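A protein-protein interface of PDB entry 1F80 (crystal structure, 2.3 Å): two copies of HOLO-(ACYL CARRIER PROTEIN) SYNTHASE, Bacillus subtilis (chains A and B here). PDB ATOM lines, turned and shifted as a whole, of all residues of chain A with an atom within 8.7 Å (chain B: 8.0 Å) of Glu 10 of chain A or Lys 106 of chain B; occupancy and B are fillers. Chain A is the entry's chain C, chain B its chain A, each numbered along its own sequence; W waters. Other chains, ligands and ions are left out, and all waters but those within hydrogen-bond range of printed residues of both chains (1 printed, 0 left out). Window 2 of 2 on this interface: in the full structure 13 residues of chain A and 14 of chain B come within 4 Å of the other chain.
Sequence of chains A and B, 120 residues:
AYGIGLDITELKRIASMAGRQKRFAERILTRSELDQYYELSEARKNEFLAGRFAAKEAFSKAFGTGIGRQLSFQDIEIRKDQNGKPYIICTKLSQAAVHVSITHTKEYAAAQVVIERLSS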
ATOM      1  N   ASP A   7      10.664  11.311  12.446  1.00  0.00           N
ATOM      2  CA  ASP A   7       9.857  11.646  11.273  1.00  0.00           C
ATOM      3  C   ASP A   7       9.310  13.061  11.356  1.00  0.00           C
ATOM      4  O   ASP A   7       8.965  13.518  12.433  1.00  0.00           O
ATOM      5  CB  ASP A   7       8.686  10.689  11.037  1.00  0.00           C
ATOM      6  CG  ASP A   7       7.857  11.108   9.791  1.00  0.00           C
ATOM      7  OD1 ASP A   7       6.782  11.742   9.961  1.00  0.00           O
ATOM      8  OD2 ASP A   7       8.302  10.845   8.626  1.00  0.00           O
ATOM      9  N   ILE A   8       9.252  13.742  10.217  1.00  0.00           N
ATOM     10  CA  ILE A   8       8.720  15.087  10.115  1.00  0.00           C
ATOM     11  C   ILE A   8       7.671  15.091   8.968  1.00  0.00           C
ATOM     12  O   ILE A   8       8.030  14.904   7.802  1.00  0.00           O
ATOM     13  CB  ILE A   8       9.822  16.124   9.780  1.00  0.00           C
ATOM     14  CG1 ILE A   8      10.922  16.141  10.843  1.00  0.00           C
ATOM     15  CG2 ILE A   8       9.204  17.513   9.731  1.00  0.00           C
ATOM     16  CD1 ILE A   8      12.147  16.994  10.427  1.00  0.00           C
ATOM     17  N   THR A   9       6.398  15.318   9.285  1.00  0.00           N
ATOM     18  CA  THR A   9       5.335  15.329   8.275  1.00  0.00           C
ATOM     19  C   THR A   9       4.677  16.704   8.070  1.00  0.00           C
ATOM     20  O   THR A   9       4.311  17.379   9.034  1.00  0.00           O
ATOM     21  CB  THR A   9       4.201  14.355   8.677  1.00  0.00           C
ATOM     22  OG1 THR A   9       4.661  12.996   8.567  1.00  0.00           O
ATOM     23  CG2 THR A   9       2.974  14.574   7.805  1.00  0.00           C
ATOM     24  N   GLU A  10       4.461  17.094   6.820  1.00  0.00           N
ATOM     25  CA  GLU A  10       3.838  18.389   6.554  1.00  0.00           C
ATOM     26  C   GLU A  10       2.376  18.343   6.868  1.00  0.00           C
ATOM     27  O   GLU A  10       1.634  17.478   6.393  1.00  0.00           O
ATOM     28  CB  GLU A  10       3.999  18.809   5.117  1.00  0.00           C
ATOM     29  CG  GLU A  10       5.425  18.946   4.698  1.00  0.00           C
ATOM     30  CD  GLU A  10       5.818  17.907   3.665  1.00  0.00           C
ATOM     31  OE1 GLU A  10       5.764  16.683   3.987  1.00  0.00           O
ATOM     32  OE2 GLU A  10       6.185  18.316   2.534  1.00  0.00           O
ATOM     33  N   LEU A  11       1.966  19.285   7.697  1.00  0.00           N
ATOM     34  CA  LEU A  11       0.581  19.393   8.105  1.00  0.00           C
ATOM     35  C   LEU A  11      -0.438  19.596   6.936  1.00  0.00           C
ATOM     36  O   LEU A  11      -1.505  19.004   6.950  1.00  0.00           O
ATOM     37  CB  LEU A  11       0.478  20.531   9.138  1.00  0.00           C
ATOM     38  CG  LEU A  11      -0.769  20.610  10.008  1.00  0.00           C
ATOM     39  CD1 LEU A  11      -0.994  19.268  10.694  1.00  0.00           C
ATOM     40  CD2 LEU A  11      -0.597  21.723  11.042  1.00  0.00           C
ATOM     41  N   LYS A  12      -0.115  20.433   5.955  1.00  0.00           N
ATOM     42  CA  LYS A  12      -1.014  20.678   4.830  1.00  0.00           C
ATOM     43  C   LYS A  12      -1.471  19.361   4.185  1.00  0.00           C
ATOM     44  O   LYS A  12      -2.651  19.124   4.002  1.00  0.00           O
ATOM     45  CB  LYS A  12      -0.343  21.585   3.761  1.00  0.00           C
ATOM     46  CG  LYS A  12       0.737  20.887   2.933  1.00  0.00           C
ATOM     47  CD  LYS A  12       1.595  21.815   2.045  1.00  0.00           C
ATOM     48  CE  LYS A  12       0.902  22.190   0.704  1.00  0.00           C
ATOM     49  NZ  LYS A  12       1.768  22.997  -0.243  1.00  0.00           N
ATOM     50  N   ARG A  13      -0.526  18.495   3.861  1.00  0.00           N
ATOM     51  CA  ARG A  13      -0.839  17.232   3.231  1.00  0.00           C
ATOM     52  C   ARG A  13      -1.822  16.397   4.029  1.00  0.00           C
ATOM     53  O   ARG A  13      -2.638  15.698   3.451  1.00  0.00           O
ATOM     54  CB  ARG A  13       0.445  16.452   3.013  1.00  0.00           C
ATOM     55  CG  ARG A  13       1.504  17.274   2.324  1.00  0.00           C
ATOM     56  CD  ARG A  13       2.810  16.511   2.299  1.00  0.00           C
ATOM     57  NE  ARG A  13       2.701  15.271   1.542  1.00  0.00           N
ATOM     58  CZ  ARG A  13       3.533  14.245   1.680  1.00  0.00           C
ATOM     59  NH1 ARG A  13       4.530  14.309   2.547  1.00  0.00           N
ATOM     60  NH2 ARG A  13       3.367  13.137   0.961  1.00  0.00           N
ATOM     61  N   ILE A  14      -1.768  16.473   5.350  1.00  0.00           N
ATOM     62  CA  ILE A  14      -2.667  15.664   6.151  1.00  0.00           C
ATOM     63  C   ILE A  14      -4.034  16.300   6.372  1.00  0.00           C
ATOM     64  O   ILE A  14      -5.017  15.612   6.639  1.00  0.00           O
ATOM     65  CB  ILE A  14      -1.992  15.272   7.494  1.00  0.00           C
ATOM     66  CG1 ILE A  14      -1.029  14.108   7.232  1.00  0.00           C
ATOM     67  CG2 ILE A  14      -3.028  14.869   8.530  1.00  0.00           C
ATOM     68  CD1 ILE A  14      -0.318  13.583   8.438  1.00  0.00           C
ATOM     69  N   ALA A  15      -4.106  17.613   6.249  1.00  0.00           N
ATOM     70  CA  ALA A  15      -5.374  18.294   6.419  1.00  0.00           C
ATOM     71  C   ALA A  15      -6.028  18.265   5.048  1.00  0.00           C
ATOM     72  O   ALA A  15      -7.245  18.107   4.942  1.00  0.00           O
ATOM     73  CB  ALA A  15      -5.146  19.727   6.863  1.00  0.00           C
ATOM     74  N   SER A  16      -5.183  18.392   4.016  1.00  0.00           N
ATOM     75  CA  SER A  16      -5.571  18.419   2.606  1.00  0.00           C
ATOM     76  C   SER A  16      -6.430  17.248   2.165  1.00  0.00           C
ATOM     77  O   SER A  16      -6.915  17.244   1.028  1.00  0.00           O
ATOM     78  CB  SER A  16      -4.323  18.443   1.698  1.00  0.00           C
ATOM     79  OG  SER A  16      -3.639  19.685   1.716  1.00  0.00           O
ATOM     80  N   MET A  17      -6.591  16.250   3.035  1.00  0.00           N
ATOM     81  CA  MET A  17      -7.405  15.071   2.715  1.00  0.00           C
ATOM     82  C   MET A  17      -8.910  15.345   2.877  1.00  0.00           C
ATOM     83  O   MET A  17      -9.506  15.058   3.912  1.00  0.00           O
ATOM     84  CB  MET A  17      -6.988  13.908   3.604  1.00  0.00           C
ATOM     85  CG  MET A  17      -5.507  13.668   3.597  1.00  0.00           C
ATOM     86  SD  MET A  17      -5.044  12.289   4.656  1.00  0.00           S
ATOM     87  CE  MET A  17      -4.441  11.107   3.391  1.00  0.00           C
ATOM     88  N   ASN A  46      -6.569  17.791  12.456  1.00  0.00           N
ATOM     89  CA  ASN A  46      -5.443  17.657  11.535  1.00  0.00           C
ATOM     90  C   ASN A  46      -4.130  17.504  12.309  1.00  0.00           C
ATOM     91  O   ASN A  46      -3.244  16.764  11.896  1.00  0.00           O
ATOM     92  CB  ASN A  46      -5.327  18.858  10.579  1.00  0.00           C
ATOM     93  CG  ASN A  46      -6.565  19.043   9.684  1.00  0.00           C
ATOM     94  OD1 ASN A  46      -7.302  18.100   9.388  1.00  0.00           O
ATOM     95  ND2 ASN A  46      -6.775  20.271   9.238  1.00  0.00           N
ATOM     96  N   LEU A  49      -3.823  13.950  14.044  1.00  0.00           N
ATOM     97  CA  LEU A  49      -3.587  12.975  12.983  1.00  0.00           C
ATOM     98  C   LEU A  49      -2.162  13.055  12.451  1.00  0.00           C
ATOM     99  O   LEU A  49      -1.528  12.037  12.276  1.00  0.00           O
ATOM    100  CB  LEU A  49      -4.588  13.231  11.859  1.00  0.00           C
ATOM    101  CG  LEU A  49      -4.988  12.158  10.867  1.00  0.00           C
ATOM    102  CD1 LEU A  49      -5.215  10.833  11.573  1.00  0.00           C
ATOM    103  CD2 LEU A  49      -6.262  12.657  10.149  1.00  0.00           C
ATOM    104  N   ALA A  50      -1.665  14.253  12.193  1.00  0.00           N
ATOM    105  CA  ALA A  50      -0.286  14.400  11.723  1.00  0.00           C
ATOM    106  C   ALA A  50       0.701  13.901  12.803  1.00  0.00           C
ATOM    107  O   ALA A  50       1.739  13.360  12.479  1.00  0.00           O
ATOM    108  CB  ALA A  50       0.014  15.867  11.389  1.00  0.00           C
ATOM    109  N   GLY A  51       0.363  14.091  14.075  1.00  0.00           N
ATOM    110  CA  GLY A  51       1.253  13.655  15.126  1.00  0.00           C
ATOM    111  C   GLY A  51       1.253  12.136  15.268  1.00  0.00           C
ATOM    112  O   GLY A  51       2.297  11.527  15.493  1.00  0.00           O
ATOM    113  N   PHE A  53       0.564  10.084  12.879  1.00  0.00           N
ATOM    114  CA  PHE A  53       1.247   9.550  11.736  1.00  0.00           C
ATOM    115  C   PHE A  53       2.772   9.676  11.916  1.00  0.00           C
ATOM    116  O   PHE A  53       3.531   8.722  11.615  1.00  0.00           O
ATOM    117  CB  PHE A  53       0.819  10.273  10.472  1.00  0.00           C
ATOM    118  CG  PHE A  53       1.483   9.740   9.213  1.00  0.00           C
ATOM    119  CD1 PHE A  53       2.564  10.385   8.659  1.00  0.00           C
ATOM    120  CD2 PHE A  53       0.972   8.624   8.557  1.00  0.00           C
ATOM    121  CE1 PHE A  53       3.129   9.961   7.466  1.00  0.00           C
ATOM    122  CE2 PHE A  53       1.536   8.186   7.361  1.00  0.00           C
ATOM    123  CZ  PHE A  53       2.614   8.861   6.813  1.00  0.00           C
ATOM    124  N   ALA A  54       3.224  10.837  12.408  1.00  0.00           N
ATOM    125  CA  ALA A  54       4.656  11.036  12.601  1.00  0.00           C
ATOM    126  C   ALA A  54       5.206  10.068  13.638  1.00  0.00           C
ATOM    127  O   ALA A  54       6.259   9.462  13.460  1.00  0.00           O
ATOM    128  CB  ALA A  54       4.940  12.475  13.037  1.00  0.00           C
ATOM    129  N   THR A 105       4.364  22.563  14.839  1.00  0.00           N
ATOM    130  CA  THR A 105       4.696  23.878  14.373  1.00  0.00           C
ATOM    131  C   THR A 105       3.501  24.241  13.447  1.00  0.00           C
ATOM    132  O   THR A 105       2.549  23.455  13.318  1.00  0.00           O
ATOM    133  CB  THR A 105       6.024  23.780  13.621  1.00  0.00           C
ATOM    134  OG1 THR A 105       6.846  24.905  13.927  1.00  0.00           O
ATOM    135  CG2 THR A 105       5.791  23.683  12.169  1.00  0.00           C
ATOM    136  N   LYS A 106       3.523  25.410  12.807  1.00  0.00           N
ATOM    137  CA  LYS A 106       2.406  25.781  11.943  1.00  0.00           C
ATOM    138  C   LYS A 106       2.408  24.881  10.717  1.00  0.00           C
ATOM    139  O   LYS A 106       1.370  24.430  10.283  1.00  0.00           O
ATOM    140  CB  LYS A 106       2.523  27.253  11.516  1.00  0.00           C
ATOM    141  N   GLU A 107       3.584  24.617  10.163  1.00  0.00           N
ATOM    142  CA  GLU A 107       3.692  23.762   8.986  1.00  0.00           C
ATOM    143  C   GLU A 107       3.941  22.280   9.240  1.00  0.00           C
ATOM    144  O   GLU A 107       3.663  21.460   8.371  1.00  0.00           O
ATOM    145  CB  GLU A 107       4.829  24.245   8.091  1.00  0.00           C
ATOM    146  CG  GLU A 107       4.658  25.664   7.545  1.00  0.00           C
ATOM    147  CD  GLU A 107       4.948  25.753   6.052  1.00  0.00           C
ATOM    148  OE1 GLU A 107       4.526  26.768   5.448  1.00  0.00           O
ATOM    149  OE2 GLU A 107       5.592  24.820   5.486  1.00  0.00           O
ATOM    150  N   TYR A 108       4.442  21.921  10.419  1.00  0.00           N
ATOM    151  CA  TYR A 108       4.940  20.550  10.445  1.00  0.00           C
ATOM    152  C   TYR A 108       4.487  19.818  11.714  1.00  0.00           C
ATOM    153  O   TYR A 108       4.167  20.417  12.732  1.00  0.00           O
ATOM    154  CB  TYR A 108       6.473  20.598  10.406  1.00  0.00           C
ATOM    155  CG  TYR A 108       6.959  21.053   9.070  1.00  0.00           C
ATOM    156  CD1 TYR A 108       6.941  20.175   7.991  1.00  0.00           C
ATOM    157  CD2 TYR A 108       7.547  22.312   8.922  1.00  0.00           C
ATOM    158  CE1 TYR A 108       7.515  20.542   6.783  1.00  0.00           C
ATOM    159  CE2 TYR A 108       8.122  22.682   7.711  1.00  0.00           C
ATOM    160  CZ  TYR A 108       8.107  21.798   6.647  1.00  0.00           C
ATOM    161  OH  TYR A 108       8.721  22.126   5.450  1.00  0.00           O
ATOM    162  N   ALA A 109       4.423  18.478  11.600  1.00  0.00           N
ATOM    163  CA  ALA A 109       4.299  17.641  12.789  1.00  0.00           C
ATOM    164  C   ALA A 109       5.449  16.632  12.838  1.00  0.00           C
ATOM    165  O   ALA A 109       5.713  15.887  11.898  1.00  0.00           O
ATOM    166  CB  ALA A 109       2.955  16.913  12.753  1.00  0.00           C
ATOM    167  N   ALA A 110       6.169  16.662  13.971  1.00  0.00           N
ATOM    168  CA  ALA A 110       7.413  15.907  14.051  1.00  0.00           C
ATOM    169  C   ALA A 110       7.433  14.948  15.244  1.00  0.00           C
ATOM    170  O   ALA A 110       6.777  15.158  16.256  1.00  0.00           O
ATOM    171  CB  ALA A 110       8.562  16.912  14.170  1.00  0.00           C
ATOM    172  N   THR B   9      18.598  20.062   7.041  1.00  0.00           N
ATOM    173  CA  THR B   9      19.229  20.721   5.897  1.00  0.00           C
ATOM    174  C   THR B   9      18.184  20.955   4.802  1.00  0.00           C
ATOM    175  O   THR B   9      17.509  20.011   4.368  1.00  0.00           O
ATOM    176  CB  THR B   9      20.321  19.825   5.289  1.00  0.00           C
ATOM    177  OG1 THR B   9      21.475  19.816   6.139  1.00  0.00           O
ATOM    178  CG2 THR B   9      20.695  20.313   3.918  1.00  0.00           C
ATOM    179  N   GLU B  10      18.073  22.208   4.373  1.00  0.00           N
ATOM    180  CA  GLU B  10      17.149  22.643   3.321  1.00  0.00           C
ATOM    181  C   GLU B  10      17.569  22.081   1.960  1.00  0.00           C
ATOM    182  O   GLU B  10      18.707  22.268   1.549  1.00  0.00           O
ATOM    183  CB  GLU B  10      17.156  24.169   3.256  1.00  0.00           C
ATOM    184  CG  GLU B  10      16.685  24.798   4.580  1.00  0.00           C
ATOM    185  CD  GLU B  10      16.976  26.301   4.732  1.00  0.00           C
ATOM    186  OE1 GLU B  10      18.137  26.700   5.066  1.00  0.00           O
ATOM    187  OE2 GLU B  10      16.023  27.087   4.519  1.00  0.00           O
ATOM    188  N   LEU B  11      16.659  21.363   1.304  1.00  0.00           N
ATOM    189  CA  LEU B  11      16.877  20.790  -0.031  1.00  0.00           C
ATOM    190  C   LEU B  11      17.343  21.803  -1.100  1.00  0.00           C
ATOM    191  O   LEU B  11      18.195  21.492  -1.953  1.00  0.00           O
ATOM    192  CB  LEU B  11      15.564  20.163  -0.549  1.00  0.00           C
ATOM    193  CG  LEU B  11      15.392  18.666  -0.763  1.00  0.00           C
ATOM    194  CD1 LEU B  11      14.145  18.440  -1.593  1.00  0.00           C
ATOM    195  CD2 LEU B  11      16.586  18.094  -1.500  1.00  0.00           C
ATOM    196  N   LYS B  12      16.747  22.999  -1.084  1.00  0.00           N
ATOM    197  CA  LYS B  12      17.062  24.048  -2.071  1.00  0.00           C
ATOM    198  C   LYS B  12      18.523  24.413  -2.053  1.00  0.00           C
ATOM    199  O   LYS B  12      19.113  24.633  -3.090  1.00  0.00           O
ATOM    200  CB  LYS B  12      16.191  25.331  -1.815  1.00  0.00           C
ATOM    201  N   GLU B  47      18.069  14.944  -3.163  1.00  0.00           N
ATOM    202  CA  GLU B  47      17.526  14.374  -1.949  1.00  0.00           C
ATOM    203  C   GLU B  47      18.558  13.493  -1.254  1.00  0.00           C
ATOM    204  O   GLU B  47      18.737  13.574  -0.033  1.00  0.00           O
ATOM    205  CB  GLU B  47      16.322  13.509  -2.246  1.00  0.00           C
ATOM    206  CG  GLU B  47      15.014  14.218  -2.275  1.00  0.00           C
ATOM    207  CD  GLU B  47      14.056  13.430  -3.118  1.00  0.00           C
ATOM    208  OE1 GLU B  47      13.885  12.212  -2.815  1.00  0.00           O
ATOM    209  OE2 GLU B  47      13.506  14.027  -4.088  1.00  0.00           O
ATOM    210  N   HIS B 104      12.611  12.916   5.296  1.00  0.00           N
ATOM    211  CA  HIS B 104      12.554  13.929   4.254  1.00  0.00           C
ATOM    212  C   HIS B 104      11.185  14.614   4.184  1.00  0.00           C
ATOM    213  O   HIS B 104      10.136  13.984   4.281  1.00  0.00           O
ATOM    214  CB  HIS B 104      12.804  13.227   2.921  1.00  0.00           C
ATOM    215  CG  HIS B 104      14.257  12.862   2.797  1.00  0.00           C
ATOM    216  ND1 HIS B 104      15.186  13.702   2.277  1.00  0.00           N
ATOM    217  CD2 HIS B 104      14.855  11.620   3.023  1.00  0.00           C
ATOM    218  CE1 HIS B 104      16.322  12.981   2.190  1.00  0.00           C
ATOM    219  NE2 HIS B 104      16.152  11.731   2.631  1.00  0.00           N
ATOM    220  N   THR B 105      11.220  15.952   4.051  1.00  0.00           N
ATOM    221  CA  THR B 105      10.036  16.649   3.554  1.00  0.00           C
ATOM    222  C   THR B 105      10.334  17.221   2.173  1.00  0.00           C
ATOM    223  O   THR B 105      11.420  17.071   1.628  1.00  0.00           O
ATOM    224  CB  THR B 105       9.662  17.770   4.520  1.00  0.00           C
ATOM    225  OG1 THR B 105      10.727  18.717   4.570  1.00  0.00           O
ATOM    226  CG2 THR B 105       9.433  17.205   5.922  1.00  0.00           C
ATOM    227  N   LYS B 106       9.320  17.854   1.571  1.00  0.00           N
ATOM    228  CA  LYS B 106       9.574  18.424   0.261  1.00  0.00           C
ATOM    229  C   LYS B 106      10.745  19.403   0.315  1.00  0.00           C
ATOM    230  O   LYS B 106      11.548  19.503  -0.608  1.00  0.00           O
ATOM    231  CB  LYS B 106       8.306  19.119  -0.233  1.00  0.00           C
ATOM    232  CG  LYS B 106       7.131  18.149  -0.359  1.00  0.00           C
ATOM    233  CD  LYS B 106       7.595  16.721  -0.640  1.00  0.00           C
ATOM    234  CE  LYS B 106       6.613  15.669  -0.122  1.00  0.00           C
ATOM    235  NZ  LYS B 106       6.264  15.961   1.265  1.00  0.00           N
ATOM    236  N   GLU B 107      10.858  20.163   1.393  1.00  0.00           N
ATOM    237  CA  GLU B 107      11.931  21.145   1.483  1.00  0.00           C
ATOM    238  C   GLU B 107      13.122  20.742   2.346  1.00  0.00           C
ATOM    239  O   GLU B 107      14.190  21.345   2.259  1.00  0.00           O
ATOM    240  CB  GLU B 107      11.368  22.457   1.997  1.00  0.00           C
ATOM    241  CG  GLU B 107      10.539  23.227   0.952  1.00  0.00           C
ATOM    242  CD  GLU B 107       9.626  24.205   1.624  1.00  0.00           C
ATOM    243  OE1 GLU B 107       8.586  24.561   1.019  1.00  0.00           O
ATOM    244  OE2 GLU B 107       9.943  24.604   2.767  1.00  0.00           O
ATOM    245  N   TYR B 108      12.978  19.695   3.137  1.00  0.00           N
ATOM    246  CA  TYR B 108      14.087  19.323   4.027  1.00  0.00           C
ATOM    247  C   TYR B 108      14.556  17.891   4.112  1.00  0.00           C
ATOM    248  O   TYR B 108      13.787  16.948   3.889  1.00  0.00           O
ATOM    249  CB  TYR B 108      13.747  19.695   5.481  1.00  0.00           C
ATOM    250  CG  TYR B 108      13.401  21.131   5.721  1.00  0.00           C
ATOM    251  CD1 TYR B 108      14.366  22.118   5.661  1.00  0.00           C
ATOM    252  CD2 TYR B 108      12.090  21.500   5.973  1.00  0.00           C
ATOM    253  CE1 TYR B 108      14.039  23.433   5.845  1.00  0.00           C
ATOM    254  CE2 TYR B 108      11.742  22.812   6.147  1.00  0.00           C
ATOM    255  CZ  TYR B 108      12.724  23.778   6.077  1.00  0.00           C
ATOM    256  OH  TYR B 108      12.358  25.091   6.164  1.00  0.00           O
ATOM    257  N   ALA B 109      15.822  17.769   4.505  1.00  0.00           N
ATOM    258  CA  ALA B 109      16.456  16.482   4.848  1.00  0.00           C
ATOM    259  C   ALA B 109      16.806  16.665   6.360  1.00  0.00           C
ATOM    260  O   ALA B 109      17.397  17.688   6.773  1.00  0.00           O
ATOM    261  CB  ALA B 109      17.702  16.273   4.068  1.00  0.00           C
HETATM  262  O   HOH W   1       8.108  20.438   3.089  1.00  0.00           O
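The side-chain amino group of Lys 106 of chain B is in salt-bridge range of the side-chain carboxylate of Glu 10 of chain A (2.7 Å). NH1 of Arg 13 of chain A lies close to NZ of Lys 106 of chain B (2.7 Å).
The side-chain hydroxyl (OG1) of Thr 105 of chain B lies close to the backbone NH (N) of Glu 107 of chain B, 3.5 Å away. The side-chain hydroxyl (OG1) of Thr 105 of chain B lies within hydrogen-bond range of the backbone NH (N) of Tyr 108 of chain B, at 2.8 Å. The backbone carbonyl oxygen (O) of Glu 107 of chain B is in hydrogen-bond range of the backbone NH (N) of Leu 11 of chain B, at 2.6 Å. OE1 of Glu 10 of chain A is in salt-bridge range of NH1 of Arg 13 of chain A, 3.0 Å away.
Among the printed residues, merely in contact across the chains: Tyr 108 of chain A with Tyr 108 of chain B, Ile 8 of chain A with Thr 105 of chain B, Tyr 108 of chain A with Glu 107 of chain B, Glu 10 of chain A with Thr 105 of chain B and Tyr 108 of chain A with Thr 105 of chain B.
Of the printed residues of chain B, Ile 8 of chain A touches Thr 105. Of chain B, only Thr 105 (3.9 Å) and Lys 106 (2.7 Å) come within 4 Å of Glu 10 of chain A. Lys 12 of chain A touches none of the printed residues of chain B. Printed residues of chain B within 4 Å of Arg 13 of chain A: Lys 106. Ile 14 of chain A touches none of the printed residues of chain B. Printed residues of chain B within 4 Å of Tyr 108 of chain A: Thr 105 (3.9 Å), Glu 107 (3.9 Å) and Tyr 108 (3.2 Å). Thr 105 of chain B touches three residues of chain A. Lys 106 of chain B touches just these residues of chain A: Glu 10 (2.7 Å) and Arg 13 (2.7 Å). Of the printed residues of chain A, Glu 107 of chain B touches Tyr 108. Of the printed residues of chain A, Tyr 108 of chain B touches Tyr 108. The nearest printed residue of chain B that does not touch Glu 10 of chain A is His 104 of chain B (5.1 Å).
Of the 23 printed residues of chain A, 4 touch a printed residue of chain B. Hydrophobic or aromatic side chains of chain A within 4 Å of the printed part of chain B: Ile 8 and Tyr 108. Of the 11 printed residues of chain B, 4 touch a printed residue of chain A. Hydrophobic or aromatic side chains of chain B within 4 Å of the printed part of chain A: Tyr 108. Among the printed residues, 7 pairs touch across the chains.
Glu 10 of chain A touches Thr 105 of chain B, but with the chains exchanged Thr 105 of chain A does not touch Glu 10 of chain B (13.2 Å). Glu 10 of chain A touches Lys 106 of chain B, but with the chains exchanged Lys 106 of chain A does not touch Glu 10 of chain B (15.1 Å). Tyr 108 of chain A touches Thr 105 of chain B, but with the chains exchanged Thr 105 of chain A does not touch Tyr 108 of chain B (8.5 Å). Tyr 108 of chain B touches its own counterpart, Tyr 108 of chain A. Positions printed for both chains: 9, 10, 11, 12, 105, 106, 107, 108 and 109. Of the 7 pairs that touch across the chains among the printed residues, 1 has its exchanged pair printed and touching as well.
Water W1 lies within hydrogen-bond range of OE2 of Glu 10 of chain A (2.9 Å), OH of Tyr 108 of chain A (3.0 Å), N of Lys 106 of chain B (3.2 Å), N of Glu 107 of chain B (3.2 Å) and OG1 of Thr 105 of chain B (3.5 Å).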
